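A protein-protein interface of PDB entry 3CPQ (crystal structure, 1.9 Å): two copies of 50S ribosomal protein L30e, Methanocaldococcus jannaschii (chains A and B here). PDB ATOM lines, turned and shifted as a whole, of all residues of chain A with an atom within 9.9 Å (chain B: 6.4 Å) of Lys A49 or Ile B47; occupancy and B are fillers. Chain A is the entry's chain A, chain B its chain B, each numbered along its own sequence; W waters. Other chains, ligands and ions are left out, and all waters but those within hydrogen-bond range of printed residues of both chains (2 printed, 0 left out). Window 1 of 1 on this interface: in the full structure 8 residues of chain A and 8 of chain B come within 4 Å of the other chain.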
ATOM      1  N   SER A  26     -27.515  18.290 -21.806  1.00  0.00           N
ATOM      2  CA  SER A  26     -28.142  19.181 -22.775  1.00  0.00           C
ATOM      3  C   SER A  26     -29.035  18.431 -23.760  1.00  0.00           C
ATOM      4  O   SER A  26     -30.155  18.859 -24.038  1.00  0.00           O
ATOM      5  CB  SER A  26     -27.066  19.975 -23.537  1.00  0.00           C
ATOM      6  OG  SER A  26     -26.189  19.108 -24.233  1.00  0.00           O
ATOM      7  N   ILE A  30     -33.165  18.827 -23.814  1.00  0.00           N
ATOM      8  CA  ILE A  30     -33.870  19.251 -25.019  1.00  0.00           C
ATOM      9  C   ILE A  30     -34.919  18.216 -25.414  1.00  0.00           C
ATOM     10  O   ILE A  30     -36.044  18.565 -25.780  1.00  0.00           O
ATOM     11  CB  ILE A  30     -32.879  19.444 -26.198  1.00  0.00           C
ATOM     12  CG1 ILE A  30     -31.958  20.633 -25.908  1.00  0.00           C
ATOM     13  CG2 ILE A  30     -33.636  19.657 -27.500  1.00  0.00           C
ATOM     14  CD1 ILE A  30     -30.878  20.848 -26.962  1.00  0.00           C
ATOM     15  N   LEU A  43     -29.341  26.218 -17.118  1.00  0.00           N
ATOM     16  CA  LEU A  43     -28.259  26.164 -18.097  1.00  0.00           C
ATOM     17  C   LEU A  43     -26.931  26.607 -17.489  1.00  0.00           C
ATOM     18  O   LEU A  43     -26.896  27.536 -16.683  1.00  0.00           O
ATOM     19  CB  LEU A  43     -28.578  27.085 -19.280  1.00  0.00           C
ATOM     20  CG  LEU A  43     -29.871  26.834 -20.062  1.00  0.00           C
ATOM     21  CD1 LEU A  43     -29.999  27.858 -21.177  1.00  0.00           C
ATOM     22  CD2 LEU A  43     -29.858  25.428 -20.640  1.00  0.00           C
ATOM     23  N   ALA A  44     -25.845  25.945 -17.881  1.00  0.00           N
ATOM     24  CA  ALA A  44     -24.518  26.312 -17.395  1.00  0.00           C
ATOM     25  C   ALA A  44     -24.070  27.547 -18.188  1.00  0.00           C
ATOM     26  O   ALA A  44     -24.603  27.827 -19.257  1.00  0.00           O
ATOM     27  CB  ALA A  44     -23.535  25.157 -17.610  1.00  0.00           C
ATOM     28  N   GLY A  45     -23.090  28.273 -17.661  1.00  0.00           N
ATOM     29  CA  GLY A  45     -22.608  29.474 -18.321  1.00  0.00           C
ATOM     30  C   GLY A  45     -21.852  29.277 -19.623  1.00  0.00           C
ATOM     31  O   GLY A  45     -21.780  30.195 -20.439  1.00  0.00           O
ATOM     32  N   ASN A  46     -21.287  28.091 -19.831  1.00  0.00           N
ATOM     33  CA  ASN A  46     -20.528  27.834 -21.051  1.00  0.00           C
ATOM     34  C   ASN A  46     -21.232  26.867 -21.991  1.00  0.00           C
ATOM     35  O   ASN A  46     -20.595  26.162 -22.766  1.00  0.00           O
ATOM     36  CB  ASN A  46     -19.114  27.327 -20.708  1.00  0.00           C
ATOM     37  CG  ASN A  46     -19.124  26.059 -19.869  1.00  0.00           C
ATOM     38  OD1 ASN A  46     -20.171  25.612 -19.395  1.00  0.00           O
ATOM     39  ND2 ASN A  46     -17.945  25.474 -19.677  1.00  0.00           N
ATOM     40  N   ILE A  47     -22.556  26.842 -21.925  1.00  0.00           N
ATOM     41  CA  ILE A  47     -23.333  25.976 -22.795  1.00  0.00           C
ATOM     42  C   ILE A  47     -23.210  26.503 -24.233  1.00  0.00           C
ATOM     43  O   ILE A  47     -23.218  27.719 -24.458  1.00  0.00           O
ATOM     44  CB  ILE A  47     -24.823  25.980 -22.382  1.00  0.00           C
ATOM     45  CG1 ILE A  47     -25.623  25.068 -23.315  1.00  0.00           C
ATOM     46  CG2 ILE A  47     -25.371  27.407 -22.416  1.00  0.00           C
ATOM     47  CD1 ILE A  47     -27.084  24.960 -22.956  1.00  0.00           C
ATOM     48  N   PRO A  48     -23.056  25.600 -25.218  1.00  0.00           N
ATOM     49  CA  PRO A  48     -22.946  26.059 -26.608  1.00  0.00           C
ATOM     50  C   PRO A  48     -24.175  26.888 -26.962  1.00  0.00           C
ATOM     51  O   PRO A  48     -25.302  26.541 -26.596  1.00  0.00           O
ATOM     52  CB  PRO A  48     -22.871  24.757 -27.392  1.00  0.00           C
ATOM     53  CG  PRO A  48     -22.094  23.881 -26.465  1.00  0.00           C
ATOM     54  CD  PRO A  48     -22.737  24.164 -25.118  1.00  0.00           C
ATOM     55  N   LYS A  49     -23.950  27.983 -27.676  1.00  0.00           N
ATOM     56  CA  LYS A  49     -25.008  28.903 -28.065  1.00  0.00           C
ATOM     57  C   LYS A  49     -26.188  28.269 -28.799  1.00  0.00           C
ATOM     58  O   LYS A  49     -27.344  28.634 -28.560  1.00  0.00           O
ATOM     59  CB  LYS A  49     -24.417  30.021 -28.927  1.00  0.00           C
ATOM     60  CG  LYS A  49     -25.437  31.015 -29.436  1.00  0.00           C
ATOM     61  CD  LYS A  49     -24.812  31.939 -30.472  1.00  0.00           C
ATOM     62  CE  LYS A  49     -25.832  32.928 -31.003  1.00  0.00           C
ATOM     63  NZ  LYS A  49     -26.407  33.731 -29.889  1.00  0.00           N
ATOM     64  N   ASP A  50     -25.906  27.339 -29.706  1.00  0.00           N
ATOM     65  CA  ASP A  50     -26.981  26.706 -30.450  1.00  0.00           C
ATOM     66  C   ASP A  50     -27.859  25.863 -29.533  1.00  0.00           C
ATOM     67  O   ASP A  50     -29.084  25.896 -29.645  1.00  0.00           O
ATOM     68  CB  ASP A  50     -26.417  25.874 -31.611  1.00  0.00           C
ATOM     69  CG  ASP A  50     -25.474  24.782 -31.156  1.00  0.00           C
ATOM     70  OD1 ASP A  50     -24.818  24.937 -30.107  1.00  0.00           O
ATOM     71  OD2 ASP A  50     -25.381  23.763 -31.871  1.00  0.00           O
ATOM     72  N   LEU A  51     -27.239  25.130 -28.612  1.00  0.00           N
ATOM     73  CA  LEU A  51     -27.999  24.306 -27.676  1.00  0.00           C
ATOM     74  C   LEU A  51     -28.826  25.218 -26.773  1.00  0.00           C
ATOM     75  O   LEU A  51     -29.978  24.921 -26.462  1.00  0.00           O
ATOM     76  CB  LEU A  51     -27.053  23.437 -26.837  1.00  0.00           C
ATOM     77  CG  LEU A  51     -26.331  22.329 -27.613  1.00  0.00           C
ATOM     78  CD1 LEU A  51     -25.377  21.562 -26.701  1.00  0.00           C
ATOM     79  CD2 LEU A  51     -27.365  21.390 -28.204  1.00  0.00           C
ATOM     80  N   GLU A  52     -28.232  26.336 -26.364  1.00  0.00           N
ATOM     81  CA  GLU A  52     -28.912  27.306 -25.506  1.00  0.00           C
ATOM     82  C   GLU A  52     -30.180  27.806 -26.194  1.00  0.00           C
ATOM     83  O   GLU A  52     -31.249  27.881 -25.588  1.00  0.00           O
ATOM     84  CB  GLU A  52     -27.997  28.503 -25.227  1.00  0.00           C
ATOM     85  CG  GLU A  52     -28.606  29.541 -24.286  1.00  0.00           C
ATOM     86  CD  GLU A  52     -28.080  30.946 -24.535  1.00  0.00           C
ATOM     87  OE1 GLU A  52     -26.958  31.084 -25.069  1.00  0.00           O
ATOM     88  OE2 GLU A  52     -28.787  31.915 -24.185  1.00  0.00           O
ATOM     89  N   GLU A  53     -30.055  28.156 -27.469  1.00  0.00           N
ATOM     90  CA  GLU A  53     -31.197  28.656 -28.224  1.00  0.00           C
ATOM     91  C   GLU A  53     -32.244  27.572 -28.438  1.00  0.00           C
ATOM     92  O   GLU A  53     -33.443  27.841 -28.377  1.00  0.00           O
ATOM     93  CB  GLU A  53     -30.731  29.214 -29.570  1.00  0.00           C
ATOM     94  CG  GLU A  53     -29.683  30.301 -29.434  1.00  0.00           C
ATOM     95  CD  GLU A  53     -29.133  30.745 -30.774  1.00  0.00           C
ATOM     96  OE1 GLU A  53     -28.804  29.866 -31.603  1.00  0.00           O
ATOM     97  OE2 GLU A  53     -29.021  31.969 -30.994  1.00  0.00           O
ATOM     98  N   ASP A  54     -31.803  26.346 -28.692  1.00  0.00           N
ATOM     99  CA  ASP A  54     -32.752  25.257 -28.890  1.00  0.00           C
ATOM    100  C   ASP A  54     -33.555  25.052 -27.608  1.00  0.00           C
ATOM    101  O   ASP A  54     -34.782  24.980 -27.640  1.00  0.00           O
ATOM    102  CB  ASP A  54     -32.034  23.956 -29.261  1.00  0.00           C
ATOM    103  CG  ASP A  54     -31.420  24.001 -30.650  1.00  0.00           C
ATOM    104  OD1 ASP A  54     -31.791  24.894 -31.442  1.00  0.00           O
ATOM    105  OD2 ASP A  54     -30.576  23.132 -30.950  1.00  0.00           O
ATOM    106  N   VAL A  55     -32.855  24.966 -26.481  1.00  0.00           N
ATOM    107  CA  VAL A  55     -33.513  24.771 -25.193  1.00  0.00           C
ATOM    108  C   VAL A  55     -34.546  25.856 -24.912  1.00  0.00           C
ATOM    109  O   VAL A  55     -35.678  25.558 -24.544  1.00  0.00           O
ATOM    110  CB  VAL A  55     -32.492  24.759 -24.024  1.00  0.00           C
ATOM    111  CG1 VAL A  55     -33.226  24.750 -22.686  1.00  0.00           C
ATOM    112  CG2 VAL A  55     -31.597  23.534 -24.127  1.00  0.00           C
ATOM    113  N   LYS A  56     -34.152  27.113 -25.081  1.00  0.00           N
ATOM    114  CA  LYS A  56     -35.054  28.231 -24.828  1.00  0.00           C
ATOM    115  C   LYS A  56     -36.258  28.236 -25.757  1.00  0.00           C
ATOM    116  O   LYS A  56     -37.351  28.649 -25.360  1.00  0.00           O
ATOM    117  CB  LYS A  56     -34.302  29.555 -24.949  1.00  0.00           C
ATOM    118  CG  LYS A  56     -33.275  29.762 -23.853  1.00  0.00           C
ATOM    119  CD  LYS A  56     -32.568  31.095 -24.005  1.00  0.00           C
ATOM    120  CE  LYS A  56     -31.577  31.318 -22.878  1.00  0.00           C
ATOM    121  NZ  LYS A  56     -30.976  32.678 -22.961  1.00  0.00           N
ATOM    122  N   TYR A  57     -36.056  27.781 -26.990  1.00  0.00           N
ATOM    123  CA  TYR A  57     -37.141  27.730 -27.961  1.00  0.00           C
ATOM    124  C   TYR A  57     -38.198  26.726 -27.516  1.00  0.00           C
ATOM    125  O   TYR A  57     -39.369  27.073 -27.371  1.00  0.00           O
ATOM    126  CB  TYR A  57     -36.614  27.331 -29.341  1.00  0.00           C
ATOM    127  CG  TYR A  57     -37.718  27.078 -30.346  1.00  0.00           C
ATOM    128  CD1 TYR A  57     -38.519  28.124 -30.811  1.00  0.00           C
ATOM    129  CD2 TYR A  57     -37.989  25.788 -30.802  1.00  0.00           C
ATOM    130  CE1 TYR A  57     -39.564  27.891 -31.706  1.00  0.00           C
ATOM    131  CE2 TYR A  57     -39.034  25.543 -31.696  1.00  0.00           C
ATOM    132  CZ  TYR A  57     -39.816  26.600 -32.141  1.00  0.00           C
ATOM    133  OH  TYR A  57     -40.849  26.363 -33.018  1.00  0.00           O
ATOM    134  N   GLN A  68     -30.696  30.858 -16.354  1.00  0.00           N
ATOM    135  CA  GLN A  68     -29.347  30.868 -16.916  1.00  0.00           C
ATOM    136  C   GLN A  68     -28.371  31.023 -15.764  1.00  0.00           C
ATOM    137  O   GLN A  68     -28.351  32.061 -15.098  1.00  0.00           O
ATOM    138  CB  GLN A  68     -29.180  32.030 -17.906  1.00  0.00           C
ATOM    139  CG  GLN A  68     -27.782  32.128 -18.528  1.00  0.00           C
ATOM    140  CD  GLN A  68     -27.424  30.918 -19.376  1.00  0.00           C
ATOM    141  OE1 GLN A  68     -28.044  30.666 -20.406  1.00  0.00           O
ATOM    142  NE2 GLN A  68     -26.421  30.165 -18.943  1.00  0.00           N
ATOM    143  N   ALA A  87     -24.120  20.629 -18.998  1.00  0.00           N
ATOM    144  CA  ALA A  87     -24.345  21.933 -19.625  1.00  0.00           C
ATOM    145  C   ALA A  87     -25.771  22.425 -19.426  1.00  0.00           C
ATOM    146  O   ALA A  87     -26.043  23.623 -19.506  1.00  0.00           O
ATOM    147  CB  ALA A  87     -24.021  21.857 -21.116  1.00  0.00           C
ATOM    148  N   SER B  26     -11.066  30.951 -30.430  1.00  0.00           N
ATOM    149  CA  SER B  26     -11.766  31.810 -29.484  1.00  0.00           C
ATOM    150  C   SER B  26     -10.807  32.481 -28.503  1.00  0.00           C
ATOM    151  O   SER B  26     -10.921  33.679 -28.242  1.00  0.00           O
ATOM    152  CB  SER B  26     -12.821  31.001 -28.720  1.00  0.00           C
ATOM    153  OG  SER B  26     -12.217  29.943 -28.001  1.00  0.00           O
ATOM    154  N   LEU B  43     -18.252  34.631 -35.282  1.00  0.00           N
ATOM    155  CA  LEU B  43     -18.467  33.578 -34.292  1.00  0.00           C
ATOM    156  C   LEU B  43     -19.214  32.385 -34.883  1.00  0.00           C
ATOM    157  O   LEU B  43     -20.107  32.560 -35.708  1.00  0.00           O
ATOM    158  CB  LEU B  43     -19.282  34.122 -33.116  1.00  0.00           C
ATOM    159  CG  LEU B  43     -18.720  35.333 -32.366  1.00  0.00           C
ATOM    160  CD1 LEU B  43     -19.704  35.765 -31.289  1.00  0.00           C
ATOM    161  CD2 LEU B  43     -17.382  34.971 -31.748  1.00  0.00           C
ATOM    162  N   ALA B  44     -18.844  31.180 -34.459  1.00  0.00           N
ATOM    163  CA  ALA B  44     -19.517  29.970 -34.922  1.00  0.00           C
ATOM    164  C   ALA B  44     -20.846  29.878 -34.155  1.00  0.00           C
ATOM    165  O   ALA B  44     -21.002  30.494 -33.100  1.00  0.00           O
ATOM    166  CB  ALA B  44     -18.655  28.743 -34.631  1.00  0.00           C
ATOM    167  N   GLY B  45     -21.791  29.110 -34.685  1.00  0.00           N
ATOM    168  CA  GLY B  45     -23.085  28.973 -34.039  1.00  0.00           C
ATOM    169  C   GLY B  45     -23.104  28.179 -32.742  1.00  0.00           C
ATOM    170  O   GLY B  45     -24.048  28.300 -31.965  1.00  0.00           O
ATOM    171  N   ASN B  46     -22.077  27.367 -32.500  1.00  0.00           N
ATOM    172  CA  ASN B  46     -22.030  26.565 -31.281  1.00  0.00           C
ATOM    173  C   ASN B  46     -20.937  27.024 -30.329  1.00  0.00           C
ATOM    174  O   ASN B  46     -20.432  26.247 -29.529  1.00  0.00           O
ATOM    175  CB  ASN B  46     -21.860  25.071 -31.620  1.00  0.00           C
ATOM    176  CG  ASN B  46     -20.586  24.779 -32.389  1.00  0.00           C
ATOM    177  OD1 ASN B  46     -19.940  25.682 -32.921  1.00  0.00           O
ATOM    178  ND2 ASN B  46     -20.226  23.500 -32.465  1.00  0.00           N
ATOM    179  N   ILE B  47     -20.575  28.300 -30.416  1.00  0.00           N
ATOM    180  CA  ILE B  47     -19.558  28.844 -29.536  1.00  0.00           C
ATOM    181  C   ILE B  47     -20.116  28.885 -28.109  1.00  0.00           C
ATOM    182  O   ILE B  47     -21.287  29.224 -27.901  1.00  0.00           O
ATOM    183  CB  ILE B  47     -19.158  30.274 -29.967  1.00  0.00           C
ATOM    184  CG1 ILE B  47     -18.065  30.811 -29.038  1.00  0.00           C
ATOM    185  CG2 ILE B  47     -20.380  31.187 -29.951  1.00  0.00           C
ATOM    186  CD1 ILE B  47     -17.532  32.171 -29.436  1.00  0.00           C
ATOM    187  N   PRO B  48     -19.298  28.502 -27.114  1.00  0.00           N
ATOM    188  CA  PRO B  48     -19.769  28.525 -25.723  1.00  0.00           C
ATOM    189  C   PRO B  48     -20.270  29.926 -25.393  1.00  0.00           C
ATOM    190  O   PRO B  48     -19.629  30.924 -25.732  1.00  0.00           O
ATOM    191  CB  PRO B  48     -18.526  28.150 -24.934  1.00  0.00           C
ATOM    192  CG  PRO B  48     -17.843  27.182 -25.860  1.00  0.00           C
ATOM    193  CD  PRO B  48     -17.971  27.864 -27.209  1.00  0.00           C
ATOM    194  N   LYS B  49     -21.418  29.990 -24.731  1.00  0.00           N
ATOM    195  CA  LYS B  49     -22.048  31.252 -24.373  1.00  0.00           C
ATOM    196  C   LYS B  49     -21.144  32.235 -23.634  1.00  0.00           C
ATOM    197  O   LYS B  49     -21.192  33.440 -23.890  1.00  0.00           O
ATOM    198  CB  LYS B  49     -23.296  30.977 -23.529  1.00  0.00           C
ATOM    199  CG  LYS B  49     -24.056  32.218 -23.101  1.00  0.00           C
ATOM    200  CD  LYS B  49     -25.141  31.855 -22.090  1.00  0.00           C
ATOM    201  CE  LYS B  49     -25.883  33.087 -21.607  1.00  0.00           C
ATOM    202  NZ  LYS B  49     -26.523  33.805 -22.751  1.00  0.00           N
ATOM    203  N   ASP B  50     -20.333  31.731 -22.710  1.00  0.00           N
ATOM    204  CA  ASP B  50     -19.454  32.607 -21.951  1.00  0.00           C
ATOM    205  C   ASP B  50     -18.407  33.254 -22.854  1.00  0.00           C
ATOM    206  O   ASP B  50     -18.145  34.456 -22.748  1.00  0.00           O
ATOM    207  CB  ASP B  50     -18.812  31.838 -20.781  1.00  0.00           C
ATOM    208  CG  ASP B  50     -17.947  30.673 -21.232  1.00  0.00           C
ATOM    209  OD1 ASP B  50     -18.241  30.057 -22.276  1.00  0.00           O
ATOM    210  OD2 ASP B  50     -16.972  30.360 -20.519  1.00  0.00           O
ATOM    211  N   LEU B  51     -17.827  32.472 -23.758  1.00  0.00           N
ATOM    212  CA  LEU B  51     -16.833  33.005 -24.684  1.00  0.00           C
ATOM    213  C   LEU B  51     -17.505  34.026 -25.602  1.00  0.00           C
ATOM    214  O   LEU B  51     -16.933  35.072 -25.909  1.00  0.00           O
ATOM    215  CB  LEU B  51     -16.210  31.871 -25.508  1.00  0.00           C
ATOM    216  CG  LEU B  51     -15.332  30.896 -24.721  1.00  0.00           C
ATOM    217  CD1 LEU B  51     -14.887  29.744 -25.616  1.00  0.00           C
ATOM    218  CD2 LEU B  51     -14.126  31.637 -24.172  1.00  0.00           C
ATOM    219  N   GLU B  52     -18.727  33.723 -26.027  1.00  0.00           N
ATOM    220  CA  GLU B  52     -19.490  34.619 -26.901  1.00  0.00           C
ATOM    221  C   GLU B  52     -19.661  35.984 -26.238  1.00  0.00           C
ATOM    222  O   GLU B  52     -19.466  37.032 -26.862  1.00  0.00           O
ATOM    223  CB  GLU B  52     -20.877  34.034 -27.179  1.00  0.00           C
ATOM    224  CG  GLU B  52     -21.728  34.889 -28.110  1.00  0.00           C
ATOM    225  CD  GLU B  52     -23.217  34.658 -27.930  1.00  0.00           C
ATOM    226  OE1 GLU B  52     -23.600  33.605 -27.376  1.00  0.00           O
ATOM    227  OE2 GLU B  52     -24.004  35.531 -28.353  1.00  0.00           O
ATOM    228  N   GLU B  53     -20.033  35.967 -24.962  1.00  0.00           N
ATOM    229  CA  GLU B  53     -20.245  37.198 -24.218  1.00  0.00           C
ATOM    230  C   GLU B  53     -18.936  37.933 -23.987  1.00  0.00           C
ATOM    231  O   GLU B  53     -18.889  39.163 -24.059  1.00  0.00           O
ATOM    232  CB  GLU B  53     -20.935  36.889 -22.886  1.00  0.00           C
ATOM    233  CG  GLU B  53     -22.255  36.155 -23.070  1.00  0.00           C
ATOM    234  CD  GLU B  53     -22.909  35.779 -21.753  1.00  0.00           C
ATOM    235  OE1 GLU B  53     -22.217  35.208 -20.878  1.00  0.00           O
ATOM    236  OE2 GLU B  53     -24.120  36.046 -21.599  1.00  0.00           O
ATOM    237  N   VAL B  55     -16.150  37.880 -25.898  1.00  0.00           N
ATOM    238  CA  VAL B  55     -15.719  38.505 -27.143  1.00  0.00           C
ATOM    239  C   VAL B  55     -16.577  39.703 -27.534  1.00  0.00           C
ATOM    240  O   VAL B  55     -16.057  40.701 -28.027  1.00  0.00           O
ATOM    241  CB  VAL B  55     -15.685  37.491 -28.319  1.00  0.00           C
ATOM    242  CG1 VAL B  55     -17.080  37.030 -28.665  1.00  0.00           C
ATOM    243  CG2 VAL B  55     -15.024  38.134 -29.538  1.00  0.00           C
ATOM    244  N   LYS B  56     -17.885  39.614 -27.314  1.00  0.00           N
ATOM    245  CA  LYS B  56     -18.770  40.718 -27.665  1.00  0.00           C
ATOM    246  C   LYS B  56     -18.509  41.928 -26.777  1.00  0.00           C
ATOM    247  O   LYS B  56     -18.607  43.070 -27.224  1.00  0.00           O
ATOM    248  CB  LYS B  56     -20.234  40.280 -27.557  1.00  0.00           C
ATOM    249  CG  LYS B  56     -20.595  39.197 -28.560  1.00  0.00           C
ATOM    250  CD  LYS B  56     -22.025  38.698 -28.408  1.00  0.00           C
ATOM    251  CE  LYS B  56     -23.035  39.712 -28.907  1.00  0.00           C
ATOM    252  NZ  LYS B  56     -24.405  39.121 -28.967  1.00  0.00           N
ATOM    253  N   GLN B  68     -22.344  37.089 -36.119  1.00  0.00           N
ATOM    254  CA  GLN B  68     -22.695  35.792 -35.555  1.00  0.00           C
ATOM    255  C   GLN B  68     -23.073  34.885 -36.712  1.00  0.00           C
ATOM    256  O   GLN B  68     -24.063  35.137 -37.398  1.00  0.00           O
ATOM    257  CB  GLN B  68     -23.877  35.917 -34.587  1.00  0.00           C
ATOM    258  CG  GLN B  68     -24.315  34.585 -33.970  1.00  0.00           C
ATOM    259  CD  GLN B  68     -23.248  33.965 -33.082  1.00  0.00           C
ATOM    260  OE1 GLN B  68     -22.881  34.530 -32.056  1.00  0.00           O
ATOM    261  NE2 GLN B  68     -22.749  32.795 -33.476  1.00  0.00           N
ATOM    262  N   HIS B  69     -22.282  33.842 -36.937  1.00  0.00           N
ATOM    263  CA  HIS B  69     -22.566  32.914 -38.021  1.00  0.00           C
ATOM    264  C   HIS B  69     -23.482  31.825 -37.474  1.00  0.00           C
ATOM    265  O   HIS B  69     -23.680  31.726 -36.258  1.00  0.00           O
ATOM    266  CB  HIS B  69     -21.264  32.297 -38.547  1.00  0.00           C
ATOM    267  CG  HIS B  69     -21.324  31.878 -39.986  1.00  0.00           C
ATOM    268  ND1 HIS B  69     -22.471  31.396 -40.579  1.00  0.00           N
ATOM    269  CD2 HIS B  69     -20.365  31.845 -40.942  1.00  0.00           C
ATOM    270  CE1 HIS B  69     -22.216  31.086 -41.839  1.00  0.00           C
ATOM    271  NE2 HIS B  69     -20.945  31.349 -42.084  1.00  0.00           N
ATOM    272  N   SER B  73     -18.575  25.222 -35.278  1.00  0.00           N
ATOM    273  CA  SER B  73     -17.144  25.504 -35.205  1.00  0.00           C
ATOM    274  C   SER B  73     -16.337  24.585 -36.130  1.00  0.00           C
ATOM    275  O   SER B  73     -15.336  25.016 -36.709  1.00  0.00           O
ATOM    276  CB  SER B  73     -16.654  25.387 -33.757  1.00  0.00           C
ATOM    277  OG  SER B  73     -16.929  24.111 -33.225  1.00  0.00           O
ATOM    278  N   ALA B  87     -14.126  28.217 -33.235  1.00  0.00           N
ATOM    279  CA  ALA B  87     -15.340  28.762 -32.632  1.00  0.00           C
ATOM    280  C   ALA B  87     -15.463  30.266 -32.846  1.00  0.00           C
ATOM    281  O   ALA B  87     -16.551  30.826 -32.758  1.00  0.00           O
ATOM    282  CB  ALA B  87     -15.372  28.436 -31.139  1.00  0.00           C
ATOM    283  N   ALA B  88     -14.331  30.907 -33.116  1.00  0.00           N
ATOM    284  CA  ALA B  88     -14.292  32.343 -33.371  1.00  0.00           C
ATOM    285  C   ALA B  88     -13.025  32.658 -34.146  1.00  0.00           C
ATOM    286  O   ALA B  88     -12.022  31.946 -34.028  1.00  0.00           O
ATOM    287  CB  ALA B  88     -14.291  33.119 -32.061  1.00  0.00           C
HETATM  288  O   HOH W   1     -26.034  33.281 -26.267  1.00  0.00           O
HETATM  289  O   HOH W   2     -15.726  27.780 -20.491  1.00  0.00           O
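Lys B49 touches Gly A45. Asn A46 touches Pro B48 (O to CB, 3.6 Å). Asn A46 touches Asp B50. O of Ile A47 touches CA of Pro B48, at 3.8 Å. Pro A48 touches Asn B46 (CB to O, 3.6 Å). O of Ile B47 touches CA of Pro A48, 3.8 Å away. Lys A49 touches Gly B45. Lys A49 touches Gln B68. Asp A50 touches Asn B46 (OD1 to CB, 3.3 Å). OE1 of Gln A68 touches CE of Lys B49, at 3.5 Å.
Gly A45 touches Lys B49, and with the chains exchanged Lys A49 touches Gly B45. Ile A47 touches Lys B49, and with the chains exchanged Lys A49 touches Ile B47. Lys A49 touches Glu B52, and with the chains exchanged Glu A52 touches Lys B49. Lys A49 touches Gln B68, and with the chains exchanged Gln A68 touches Lys B49. 16 positions are printed for both chains. Of the 16 pairs that touch across the chains among the printed residues, 16 have their exchanged pair printed and touching as well.
Lys A49 touches just these residues of chain B: Gly B45 (3.5 Å), Ile B47 (2.9 Å), Glu B52 (3.4 Å) and Gln B68 (3.5 Å). Ile B47 touches just these residues of chain A: Pro A48 (3.8 Å) and Lys A49 (2.9 Å). No residue of chain A comes within 4 Å of Ala B44. Pro B48 touches just these residues of chain A: Asn A46 (3.6 Å) and Ile A47 (3.8 Å). Of the printed residues of chain A, Glu B52 touches Lys A49. Printed residues of chain B within 4 Å of Ile A47: Pro B48 and Lys B49. Of the printed residues of chain B, Gly A45 touches Lys B49 and Asp B50. Printed residues of chain B within 4 Å of Gln A68: Lys B49. Printed residues of chain A within 4 Å of Gln B68: Lys A49. Of the printed residues of chain B, Pro A48 touches Asn B46 and Ile B47. Leu B43 touches none of the printed residues of chain A. Leu B51 touches none of the printed residues of chain A. The nearest residue of chain B that does not touch Lys A49 is Asn B46 (4.1 Å). The nearest residue of chain A that does not touch Ile B47 is Ile A47 (4.2 Å). The nearest printed residue of chain A that does not touch Gln B68 is Glu A53 (6.2 Å).
Water W1 bridges the side-chain carboxylate (OE1) of Glu A52 (2.7 Å) and the side-chain carboxylate (OE1) of Glu B52 (2.7 Å). Water W2 bridges the side-chain carboxylate (OD2) of Asp B50 (2.9 Å) and the side-chain amide nitrogen (ND2) of Asn A46 (3.3 Å).
Printed residues of chain B that touch a printed residue of chain A: Gly B45, Asn B46, Ile B47, Pro B48, Lys B49, Asp B50, Glu B52 and Gln B68. Of the 19 printed residues of chain A, 8 touch a printed residue of chain B. Printed residues of chain A that touch a printed residue of chain B: Gly A45, Asn A46, Ile A47, Pro A48, Lys A49, Asp A50, Glu A52 and Gln A68. Hydrophobic or aromatic side chains of chain A that line the printed part of chain B: Pro A48. Along chain A the printed residues that touch a printed residue of chain B span positions 45 to 68. Among the printed residues, 16 pairs touch across the chains. Among the printed residues, Asp or Glu carboxylates within 4 Å of a Lys or Arg side-chain nitrogen of the other chain: Lys A49 with Glu B52 (3.4 Å) and Glu A52 with Lys B49 (3.3 Å).
NE2 of Gln A68 lies within hydrogen-bond range of O of Ala A44 (3.0 Å). The side-chain carboxylate (OE2) of Glu A53 is in salt-bridge range of the side-chain amino group (NZ) of Lys A49, 3.3 Å away. The side-chain carboxylate of Glu A52 lies within salt-bridge range of the side-chain amino group of Lys A56, at 2.6 Å. The backbone carbonyl oxygen (O) of Leu B43 sits at hydrogen-bond distance from the side-chain amide nitrogen (NE2) of Gln B68. O of Ala B44 lies within hydrogen-bond range of NE2 of Gln B68 (2.9 Å). The side-chain amide oxygen (OD1) of Asn B46 lies within hydrogen-bond range of the backbone NH (N) of Ser B73 (2.8 Å).
O of Gly A45 lies within hydrogen-bond range of N of Asp B50. N of Lys B49 sits at hydrogen-bond distance from O of Ile A47 (2.9 Å). N of Lys A49 lies within hydrogen-bond range of O of Ile B47, 2.9 Å away. The side-chain amino group (NZ) of Lys A49 lies within salt-bridge range of the side-chain carboxylate (OE2) of Glu B52, at 3.4 Å. The backbone carbonyl oxygen (O) of Gly B45 is in hydrogen-bond range of the backbone NH (N) of Asp A50 (3.1 Å). The side-chain carboxylate of Glu A52 lies within salt-bridge range of the side-chain amino group of Lys B49.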
